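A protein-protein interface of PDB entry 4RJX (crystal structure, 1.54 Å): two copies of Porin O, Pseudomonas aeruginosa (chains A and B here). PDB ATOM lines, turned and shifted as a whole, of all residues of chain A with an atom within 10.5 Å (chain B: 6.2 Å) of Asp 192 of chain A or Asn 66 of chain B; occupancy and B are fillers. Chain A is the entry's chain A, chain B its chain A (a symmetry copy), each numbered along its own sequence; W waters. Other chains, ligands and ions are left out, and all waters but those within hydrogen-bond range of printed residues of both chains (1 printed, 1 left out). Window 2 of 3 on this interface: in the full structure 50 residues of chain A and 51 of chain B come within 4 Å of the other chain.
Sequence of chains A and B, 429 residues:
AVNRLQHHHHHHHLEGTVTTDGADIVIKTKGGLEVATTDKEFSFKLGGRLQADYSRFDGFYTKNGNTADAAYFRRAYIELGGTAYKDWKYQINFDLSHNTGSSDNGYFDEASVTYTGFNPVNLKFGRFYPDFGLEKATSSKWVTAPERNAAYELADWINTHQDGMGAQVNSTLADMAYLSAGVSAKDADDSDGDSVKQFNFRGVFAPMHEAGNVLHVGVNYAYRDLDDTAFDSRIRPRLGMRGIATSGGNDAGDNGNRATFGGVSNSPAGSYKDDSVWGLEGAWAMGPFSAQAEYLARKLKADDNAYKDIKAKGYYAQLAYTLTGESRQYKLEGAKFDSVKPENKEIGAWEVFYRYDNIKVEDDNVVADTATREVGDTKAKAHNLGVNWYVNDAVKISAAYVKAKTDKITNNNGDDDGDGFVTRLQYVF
The side-chain carboxylate (OD1) of Asp 192 of chain A lies within hydrogen-bond range of the side-chain amide nitrogen (ND2) of Asn 64 of chain B, at 3.0 Å. ND2 of Asn 66 of chain B is in hydrogen-bond range of OD1 of Asp 192 of chain A (3.0 Å). The backbone carbonyl oxygen (O) of Asp 192 of chain A lies within hydrogen-bond range of the side-chain amide nitrogen (ND2) of Asn 255 of chain B, at 2.9 Å. The backbone carbonyl oxygen (O) of Gly 193 of chain A sits at hydrogen-bond distance from the backbone NH (N) of Asp 69 of chain B, 3.1 Å away. The backbone NH of Ser 195 of chain A is in hydrogen-bond range of the side-chain carboxylate of Asp 69 of chain B, at 2.8 Å. The side-chain amino group of Lys 197 of chain A lies within salt-bridge range of the side-chain carboxylate of Asp 69 of chain B. O of Ala 252 of chain B sits close to OD2 of Asp 189 of chain A. OD1 of Asp 194 of chain A lies close to OD2 of Asp 69 of chain B (3.1 Å).
Among the printed residues, pairs that only touch across the chains: Asp 192 of chain A with Ala 68 of chain B, Gly 193 of chain A with Ala 252 of chain B, Asp 192 of chain A with Thr 67 of chain B, Gly 193 of chain A with Ala 68 of chain B, Ser 191 of chain A with Asn 64 of chain B and Ser 191 of chain A with Asn 255 of chain B.
Of the 16 printed residues of chain B, 7 touch a printed residue of chain A. Among the printed residues, Asp or Glu carboxylates within 4 Å of a Lys or Arg side-chain nitrogen of the other chain: Lys 197 of chain A with Asp 69 of chain B (2.9 Å).
No position is printed for both chains. Of the 14 pairs that touch across the chains among the printed residues, none has its exchanged pair printed and touching as well.
The side-chain carboxylate (OD1) of Asp 190 of chain A lies within hydrogen-bond range of the backbone NH (N) of Gly 193 of chain A (3.2 Å). The side-chain hydroxyl (OG) of Ser 191 of chain A sits at hydrogen-bond distance from the side-chain carboxylate (OD2) of Asp 228 of chain A. The backbone carbonyl oxygen (O) of Phe 57 of chain B is in hydrogen-bond range of the backbone NH (N) of Ala 68 of chain B. The side-chain hydroxyl (OG1) of Thr 62 of chain B is in hydrogen-bond range of the backbone carbonyl oxygen (O) of Asn 66 of chain B (2.8 Å). The side-chain amide oxygen (OD1) of Asn 64 of chain B is in hydrogen-bond range of the backbone NH (N) of Asn 66 of chain B. OD1 of Asn 64 of chain B is in hydrogen-bond range of ND2 of Asn 255 of chain B (2.9 Å).
Asp 192 of chain A touches just these residues of chain B: Asn 64, Asn 66, Thr 67, Ala 68 and Asn 255. No residue of chain A comes within 4 Å of Asp 58 of chain B. No residue of chain A comes within 4 Å of Gly 59 of chain B. No residue of chain A comes within 4 Å of Thr 62 of chain B. No residue of chain A comes within 4 Å of Gly 65 of chain B. Thr 67 of chain B touches one residue of chain A. Of the printed residues of chain A, Ala 68 of chain B touches Asp 192 and Gly 193. Of the printed residues of chain A, Asn 255 of chain B touches Ser 191 (3.9 Å) and Asp 192 (2.9 Å). Printed residues of chain B within 4 Å of Gly 193 of chain A: Ala 68 (3.6 Å), Asp 69 (3.1 Å) and Ala 252 (3.3 Å). Of the printed residues of chain B, Lys 197 of chain A touches Asp 69 (2.9 Å). Of the printed residues of chain A, Asp 69 of chain B touches Gly 193 (3.1 Å), Asp 194 (3.0 Å), Ser 195 (2.8 Å) and Lys 197 (2.9 Å). Printed residues of chain B within 4 Å of Asp 189 of chain A: Ala 252. Leu 226 of chain A touches none of the printed residues of chain B. The nearest residue of chain B that does not touch Asp 192 of chain A is Ala 252 of chain B (4.8 Å).
Water W1 bridges O of Thr 67 of chain B (2.7 Å) and OD2 of Asp 192 of chain A (3.2 Å).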
ATOM      1  N   ALA A 188     -23.210  -9.972  27.795  1.00  0.00           N
ATOM      2  CA  ALA A 188     -22.129 -10.390  26.895  1.00  0.00           C
ATOM      3  C   ALA A 188     -21.452 -11.568  27.564  1.00  0.00           C
ATOM      4  O   ALA A 188     -21.145 -11.502  28.755  1.00  0.00           O
ATOM      5  CB  ALA A 188     -21.137  -9.263  26.654  1.00  0.00           C
ATOM      6  N   ASP A 189     -21.219 -12.639  26.804  1.00  0.00           N
ATOM      7  CA  ASP A 189     -20.623 -13.856  27.346  1.00  0.00           C
ATOM      8  C   ASP A 189     -19.160 -14.050  26.956  1.00  0.00           C
ATOM      9  O   ASP A 189     -18.754 -13.711  25.841  1.00  0.00           O
ATOM     10  CB  ASP A 189     -21.380 -15.091  26.855  1.00  0.00           C
ATOM     11  CG  ASP A 189     -22.699 -15.314  27.564  1.00  0.00           C
ATOM     12  OD1 ASP A 189     -22.911 -14.782  28.674  1.00  0.00           O
ATOM     13  OD2 ASP A 189     -23.518 -16.064  26.993  1.00  0.00           O
ATOM     14  N   ASP A 190     -18.380 -14.641  27.858  1.00  0.00           N
ATOM     15  CA  ASP A 190     -17.069 -15.170  27.475  1.00  0.00           C
ATOM     16  C   ASP A 190     -17.246 -16.494  26.712  1.00  0.00           C
ATOM     17  O   ASP A 190     -18.375 -16.886  26.409  1.00  0.00           O
ATOM     18  CB  ASP A 190     -16.159 -15.321  28.709  1.00  0.00           C
ATOM     19  CG  ASP A 190     -16.662 -16.353  29.733  1.00  0.00           C
ATOM     20  OD1 ASP A 190     -17.506 -17.212  29.415  1.00  0.00           O
ATOM     21  OD2 ASP A 190     -16.177 -16.305  30.883  1.00  0.00           O
ATOM     22  N   SER A 191     -16.154 -17.188  26.381  1.00  0.00           N
ATOM     23  CA  SER A 191     -16.289 -18.389  25.549  1.00  0.00           C
ATOM     24  C   SER A 191     -16.983 -19.556  26.262  1.00  0.00           C
ATOM     25  O   SER A 191     -17.396 -20.521  25.615  1.00  0.00           O
ATOM     26  CB  SER A 191     -14.916 -18.843  25.020  1.00  0.00           C
ATOM     27  OG  SER A 191     -14.098 -19.354  26.053  1.00  0.00           O
ATOM     28  N   ASP A 192     -17.129 -19.465  27.584  1.00  0.00           N
ATOM     29  CA  ASP A 192     -17.885 -20.480  28.332  1.00  0.00           C
ATOM     30  C   ASP A 192     -19.354 -20.106  28.547  1.00  0.00           C
ATOM     31  O   ASP A 192     -20.089 -20.873  29.156  1.00  0.00           O
ATOM     32  CB  ASP A 192     -17.242 -20.742  29.699  1.00  0.00           C
ATOM     33  CG  ASP A 192     -15.913 -21.477  29.595  1.00  0.00           C
ATOM     34  OD1 ASP A 192     -15.687 -22.202  28.600  1.00  0.00           O
ATOM     35  OD2 ASP A 192     -15.101 -21.336  30.528  1.00  0.00           O
ATOM     36  N   GLY A 193     -19.786 -18.948  28.052  1.00  0.00           N
ATOM     37  CA  GLY A 193     -21.166 -18.519  28.252  1.00  0.00           C
ATOM     38  C   GLY A 193     -21.398 -17.809  29.573  1.00  0.00           C
ATOM     39  O   GLY A 193     -22.544 -17.669  30.006  1.00  0.00           O
ATOM     40  N   ASP A 194     -20.318 -17.356  30.212  1.00  0.00           N
ATOM     41  CA  ASP A 194     -20.394 -16.651  31.495  1.00  0.00           C
ATOM     42  C   ASP A 194     -20.395 -15.134  31.245  1.00  0.00           C
ATOM     43  O   ASP A 194     -19.527 -14.608  30.548  1.00  0.00           O
ATOM     44  CB  ASP A 194     -19.215 -17.072  32.379  1.00  0.00           C
ATOM     45  CG  ASP A 194     -19.449 -16.835  33.856  1.00  0.00           C
ATOM     46  OD1 ASP A 194     -20.564 -16.429  34.256  1.00  0.00           O
ATOM     47  OD2 ASP A 194     -18.497 -17.088  34.625  1.00  0.00           O
ATOM     48  N   SER A 195     -21.380 -14.440  31.808  1.00  0.00           N
ATOM     49  CA  SER A 195     -21.585 -13.017  31.547  1.00  0.00           C
ATOM     50  C   SER A 195     -20.486 -12.121  32.120  1.00  0.00           C
ATOM     51  O   SER A 195     -19.816 -12.468  33.095  1.00  0.00           O
ATOM     52  CB  SER A 195     -22.940 -12.584  32.104  1.00  0.00           C
ATOM     53  OG  SER A 195     -22.942 -12.693  33.522  1.00  0.00           O
ATOM     54  N   VAL A 196     -20.306 -10.969  31.488  1.00  0.00           N
ATOM     55  CA  VAL A 196     -19.437  -9.918  32.012  1.00  0.00           C
ATOM     56  C   VAL A 196     -19.963  -9.426  33.353  1.00  0.00           C
ATOM     57  O   VAL A 196     -21.132  -9.059  33.466  1.00  0.00           O
ATOM     58  CB  VAL A 196     -19.336  -8.728  31.030  1.00  0.00           C
ATOM     59  CG1 VAL A 196     -18.637  -7.535  31.691  1.00  0.00           C
ATOM     60  CG2 VAL A 196     -18.596  -9.139  29.766  1.00  0.00           C
ATOM     61  N   LYS A 197     -19.101  -9.430  34.369  1.00  0.00           N
ATOM     62  CA  LYS A 197     -19.481  -8.908  35.681  1.00  0.00           C
ATOM     63  C   LYS A 197     -18.912  -7.509  35.900  1.00  0.00           C
ATOM     64  O   LYS A 197     -17.783  -7.210  35.491  1.00  0.00           O
ATOM     65  CB  LYS A 197     -19.014  -9.847  36.796  1.00  0.00           C
ATOM     66  CG  LYS A 197     -19.490 -11.303  36.647  1.00  0.00           C
ATOM     67  CD  LYS A 197     -21.005 -11.408  36.424  1.00  0.00           C
ATOM     68  CE  LYS A 197     -21.487 -12.856  36.522  1.00  0.00           C
ATOM     69  NZ  LYS A 197     -20.868 -13.699  35.447  1.00  0.00           N
ATOM     70  N   LEU A 226     -13.489  -8.151  31.308  1.00  0.00           N
ATOM     71  CA  LEU A 226     -13.759  -8.564  29.928  1.00  0.00           C
ATOM     72  C   LEU A 226     -12.944  -9.777  29.497  1.00  0.00           C
ATOM     73  O   LEU A 226     -12.837 -10.057  28.302  1.00  0.00           O
ATOM     74  CB  LEU A 226     -13.481  -7.409  28.957  1.00  0.00           C
ATOM     75  CG  LEU A 226     -14.320  -6.146  29.200  1.00  0.00           C
ATOM     76  CD1 LEU A 226     -13.726  -4.960  28.443  1.00  0.00           C
ATOM     77  CD2 LEU A 226     -15.761  -6.392  28.773  1.00  0.00           C
ATOM     78  N   ASP A 227     -12.373 -10.483  30.466  1.00  0.00           N
ATOM     79  CA  ASP A 227     -11.578 -11.681  30.200  1.00  0.00           C
ATOM     80  C   ASP A 227     -12.247 -12.623  29.189  1.00  0.00           C
ATOM     81  O   ASP A 227     -13.394 -13.020  29.364  1.00  0.00           O
ATOM     82  CB  ASP A 227     -11.315 -12.417  31.522  1.00  0.00           C
ATOM     83  CG  ASP A 227     -10.349 -13.573  31.375  1.00  0.00           C
ATOM     84  OD1 ASP A 227      -9.401 -13.469  30.573  1.00  0.00           O
ATOM     85  OD2 ASP A 227     -10.537 -14.587  32.077  1.00  0.00           O
ATOM     86  N   ASP A 228     -11.521 -12.963  28.120  1.00  0.00           N
ATOM     87  CA  ASP A 228     -11.984 -13.956  27.151  1.00  0.00           C
ATOM     88  C   ASP A 228     -13.359 -13.597  26.565  1.00  0.00           C
ATOM     89  O   ASP A 228     -14.167 -14.469  26.281  1.00  0.00           O
ATOM     90  CB  ASP A 228     -12.014 -15.348  27.812  1.00  0.00           C
ATOM     91  CG  ASP A 228     -12.334 -16.471  26.829  1.00  0.00           C
ATOM     92  OD1 ASP A 228     -11.777 -16.468  25.711  1.00  0.00           O
ATOM     93  OD2 ASP A 228     -13.171 -17.338  27.170  1.00  0.00           O
ATOM     94  N   THR A 229     -13.619 -12.305  26.375  1.00  0.00           N
ATOM     95  CA  THR A 229     -14.928 -11.855  25.905  1.00  0.00           C
ATOM     96  C   THR A 229     -14.812 -10.972  24.672  1.00  0.00           C
ATOM     97  O   THR A 229     -14.110  -9.960  24.689  1.00  0.00           O
ATOM     98  CB  THR A 229     -15.693 -11.071  27.010  1.00  0.00           C
ATOM     99  OG1 THR A 229     -15.774 -11.876  28.192  1.00  0.00           O
ATOM    100  CG2 THR A 229     -17.095 -10.725  26.539  1.00  0.00           C
ATOM    101  N   ALA A 230     -15.496 -11.356  23.600  1.00  0.00           N
ATOM    102  CA  ALA A 230     -15.572 -10.492  22.424  1.00  0.00           C
ATOM    103  C   ALA A 230     -16.561  -9.365  22.680  1.00  0.00           C
ATOM    104  O   ALA A 230     -17.644  -9.586  23.236  1.00  0.00           O
ATOM    105  CB  ALA A 230     -15.959 -11.293  21.180  1.00  0.00           C
ATOM    106  N   ALA A 269     -12.247 -11.973  21.626  1.00  0.00           N
ATOM    107  CA  ALA A 269     -12.043 -12.563  22.939  1.00  0.00           C
ATOM    108  C   ALA A 269     -10.552 -12.670  23.230  1.00  0.00           C
ATOM    109  O   ALA A 269      -9.787 -13.203  22.413  1.00  0.00           O
ATOM    110  CB  ALA A 269     -12.700 -13.935  23.017  1.00  0.00           C
ATOM    111  N   PHE B  57     -24.514 -23.179  35.614  1.00  0.00           N
ATOM    112  CA  PHE B  57     -24.742 -24.572  35.235  1.00  0.00           C
ATOM    113  C   PHE B  57     -23.593 -25.065  34.368  1.00  0.00           C
ATOM    114  O   PHE B  57     -22.955 -24.271  33.683  1.00  0.00           O
ATOM    115  CB  PHE B  57     -26.082 -24.707  34.503  1.00  0.00           C
ATOM    116  CG  PHE B  57     -26.349 -23.589  33.521  1.00  0.00           C
ATOM    117  CD1 PHE B  57     -25.905 -23.687  32.215  1.00  0.00           C
ATOM    118  CD2 PHE B  57     -27.010 -22.432  33.915  1.00  0.00           C
ATOM    119  CE1 PHE B  57     -26.128 -22.658  31.308  1.00  0.00           C
ATOM    120  CE2 PHE B  57     -27.231 -21.396  33.014  1.00  0.00           C
ATOM    121  CZ  PHE B  57     -26.785 -21.511  31.707  1.00  0.00           C
ATOM    122  N   ASP B  58     -23.328 -26.369  34.414  1.00  0.00           N
ATOM    123  CA  ASP B  58     -22.241 -26.957  33.623  1.00  0.00           C
ATOM    124  C   ASP B  58     -22.541 -28.406  33.222  1.00  0.00           C
ATOM    125  O   ASP B  58     -23.689 -28.854  33.281  1.00  0.00           O
ATOM    126  CB  ASP B  58     -20.910 -26.858  34.393  1.00  0.00           C
ATOM    127  CG  ASP B  58     -20.816 -27.848  35.540  1.00  0.00           C
ATOM    128  OD1 ASP B  58     -21.870 -28.250  36.041  1.00  0.00           O
ATOM    129  OD2 ASP B  58     -19.685 -28.240  35.925  1.00  0.00           O
ATOM    130  N   GLY B  59     -21.507 -29.130  32.805  1.00  0.00           N
ATOM    131  CA  GLY B  59     -21.694 -30.482  32.300  1.00  0.00           C
ATOM    132  C   GLY B  59     -22.561 -30.467  31.056  1.00  0.00           C
ATOM    133  O   GLY B  59     -22.420 -29.578  30.217  1.00  0.00           O
ATOM    134  N   THR B  62     -24.020 -27.383  29.092  1.00  0.00           N
ATOM    135  CA  THR B  62     -23.248 -26.547  28.164  1.00  0.00           C
ATOM    136  C   THR B  62     -22.532 -27.396  27.126  1.00  0.00           C
ATOM    137  O   THR B  62     -22.336 -28.595  27.318  1.00  0.00           O
ATOM    138  CB  THR B  62     -22.222 -25.649  28.901  1.00  0.00           C
ATOM    139  OG1 THR B  62     -21.174 -26.452  29.465  1.00  0.00           O
ATOM    140  CG2 THR B  62     -22.926 -24.867  30.017  1.00  0.00           C
ATOM    141  N   LYS B  63     -22.160 -26.768  26.016  1.00  0.00           N
ATOM    142  CA  LYS B  63     -21.535 -27.508  24.922  1.00  0.00           C
ATOM    143  C   LYS B  63     -20.158 -28.030  25.314  1.00  0.00           C
ATOM    144  O   LYS B  63     -19.856 -29.196  25.070  1.00  0.00           O
ATOM    145  CB  LYS B  63     -21.425 -26.640  23.665  1.00  0.00           C
ATOM    146  CG  LYS B  63     -22.769 -26.401  22.960  1.00  0.00           C
ATOM    147  CD  LYS B  63     -22.596 -25.579  21.693  1.00  0.00           C
ATOM    148  CE  LYS B  63     -23.937 -25.306  21.030  1.00  0.00           C
ATOM    149  NZ  LYS B  63     -23.833 -24.238  19.997  1.00  0.00           N
ATOM    150  N   ASN B  64     -19.326 -27.192  25.934  1.00  0.00           N
ATOM    151  CA  ASN B  64     -17.999 -27.674  26.309  1.00  0.00           C
ATOM    152  C   ASN B  64     -17.923 -28.240  27.727  1.00  0.00           C
ATOM    153  O   ASN B  64     -16.876 -28.747  28.142  1.00  0.00           O
ATOM    154  CB  ASN B  64     -16.929 -26.577  26.114  1.00  0.00           C
ATOM    155  CG  ASN B  64     -17.160 -25.334  26.967  1.00  0.00           C
ATOM    156  OD1 ASN B  64     -17.833 -25.369  27.993  1.00  0.00           O
ATOM    157  ND2 ASN B  64     -16.557 -24.225  26.544  1.00  0.00           N
ATOM    158  N   GLY B  65     -19.029 -28.171  28.466  1.00  0.00           N
ATOM    159  CA  GLY B  65     -19.062 -28.711  29.815  1.00  0.00           C
ATOM    160  C   GLY B  65     -18.623 -27.757  30.920  1.00  0.00           C
ATOM    161  O   GLY B  65     -18.804 -28.065  32.102  1.00  0.00           O
ATOM    162  N   ASN B  66     -18.050 -26.612  30.549  1.00  0.00           N
ATOM    163  CA  ASN B  66     -17.627 -25.613  31.529  1.00  0.00           C
ATOM    164  C   ASN B  66     -18.830 -24.828  32.026  1.00  0.00           C
ATOM    165  O   ASN B  66     -19.923 -24.952  31.484  1.00  0.00           O
ATOM    166  CB  ASN B  66     -16.588 -24.657  30.938  1.00  0.00           C
ATOM    167  CG  ASN B  66     -15.296 -25.357  30.571  1.00  0.00           C
ATOM    168  OD1 ASN B  66     -14.953 -26.391  31.148  1.00  0.00           O
ATOM    169  ND2 ASN B  66     -14.564 -24.790  29.618  1.00  0.00           N
ATOM    170  N   THR B  67     -18.625 -24.007  33.051  1.00  0.00           N
ATOM    171  CA  THR B  67     -19.733 -23.289  33.673  1.00  0.00           C
ATOM    172  C   THR B  67     -20.156 -22.054  32.882  1.00  0.00           C
ATOM    173  O   THR B  67     -19.338 -21.183  32.590  1.00  0.00           O
ATOM    174  CB  THR B  67     -19.365 -22.877  35.096  1.00  0.00           C
ATOM    175  OG1 THR B  67     -19.013 -24.050  35.848  1.00  0.00           O
ATOM    176  CG2 THR B  67     -20.547 -22.150  35.790  1.00  0.00           C
ATOM    177  N   ALA B  68     -21.445 -21.999  32.545  1.00  0.00           N
ATOM    178  CA  ALA B  68     -22.062 -20.816  31.957  1.00  0.00           C
ATOM    179  C   ALA B  68     -22.991 -20.184  32.979  1.00  0.00           C
ATOM    180  O   ALA B  68     -23.252 -20.784  34.022  1.00  0.00           O
ATOM    181  CB  ALA B  68     -22.840 -21.180  30.711  1.00  0.00           C
ATOM    182  N   ASP B  69     -23.502 -18.994  32.689  1.00  0.00           N
ATOM    183  CA  ASP B  69     -24.553 -18.444  33.538  1.00  0.00           C
ATOM    184  C   ASP B  69     -25.658 -17.775  32.735  1.00  0.00           C
ATOM    185  O   ASP B  69     -25.626 -17.718  31.505  1.00  0.00           O
ATOM    186  CB  ASP B  69     -23.963 -17.476  34.599  1.00  0.00           C
ATOM    187  CG  ASP B  69     -23.575 -16.108  34.045  1.00  0.00           C
ATOM    188  OD1 ASP B  69     -23.512 -15.904  32.812  1.00  0.00           O
ATOM    189  OD2 ASP B  69     -23.305 -15.211  34.875  1.00  0.00           O
ATOM    190  N   ALA B 252     -26.639 -18.518  28.161  1.00  0.00           N
ATOM    191  CA  ALA B 252     -25.373 -19.215  27.947  1.00  0.00           C
ATOM    192  C   ALA B 252     -24.789 -18.984  26.557  1.00  0.00           C
ATOM    193  O   ALA B 252     -23.685 -19.438  26.274  1.00  0.00           O
ATOM    194  CB  ALA B 252     -25.550 -20.739  28.202  1.00  0.00           C
ATOM    195  N   ASN B 255     -22.436 -21.278  24.101  1.00  0.00           N
ATOM    196  CA  ASN B 255     -22.061 -22.460  24.871  1.00  0.00           C
ATOM    197  C   ASN B 255     -23.260 -23.129  25.573  1.00  0.00           C
ATOM    198  O   ASN B 255     -23.075 -24.094  26.307  1.00  0.00           O
ATOM    199  CB  ASN B 255     -20.981 -22.122  25.912  1.00  0.00           C
ATOM    200  CG  ASN B 255     -20.224 -23.358  26.400  1.00  0.00           C
ATOM    201  OD1 ASN B 255     -19.985 -24.298  25.634  1.00  0.00           O
ATOM    202  ND2 ASN B 255     -19.844 -23.360  27.674  1.00  0.00           N
ATOM    203  N   GLY B 256     -24.481 -22.648  25.342  1.00  0.00           N
ATOM    204  CA  GLY B 256     -25.649 -23.354  25.862  1.00  0.00           C
ATOM    205  C   GLY B 256     -25.924 -24.631  25.066  1.00  0.00           C
ATOM    206  O   GLY B 256     -25.851 -24.611  23.844  1.00  0.00           O
ATOM    207  N   ASN B 411     -22.696 -33.857  25.452  1.00  0.00           N
ATOM    208  CA  ASN B 411     -22.217 -32.595  24.900  1.00  0.00           C
ATOM    209  C   ASN B 411     -20.880 -32.834  24.196  1.00  0.00           C
ATOM    210  O   ASN B 411     -20.453 -33.980  24.037  1.00  0.00           O
ATOM    211  CB  ASN B 411     -22.087 -31.512  25.989  1.00  0.00           C
ATOM    212  CG  ASN B 411     -21.078 -31.871  27.082  1.00  0.00           C
ATOM    213  OD1 ASN B 411     -20.279 -32.811  26.944  1.00  0.00           O
ATOM    214  ND2 ASN B 411     -21.100 -31.097  28.178  1.00  0.00           N
ATOM    215  N   ASP B 415     -19.796 -35.368  28.139  1.00  0.00           N
ATOM    216  CA  ASP B 415     -20.521 -35.434  29.412  1.00  0.00           C
ATOM    217  C   ASP B 415     -21.898 -36.070  29.244  1.00  0.00           C
ATOM    218  O   ASP B 415     -22.648 -35.694  28.343  1.00  0.00           O
ATOM    219  CB  ASP B 415     -20.709 -34.044  30.034  1.00  0.00           C
ATOM    220  CG  ASP B 415     -19.403 -33.345  30.342  1.00  0.00           C
ATOM    221  OD1 ASP B 415     -18.386 -34.022  30.629  1.00  0.00           O
ATOM    222  OD2 ASP B 415     -19.407 -32.099  30.305  1.00  0.00           O
HETATM  223  O   HOH W   1     -16.758 -20.673  33.191  1.00  0.00           O
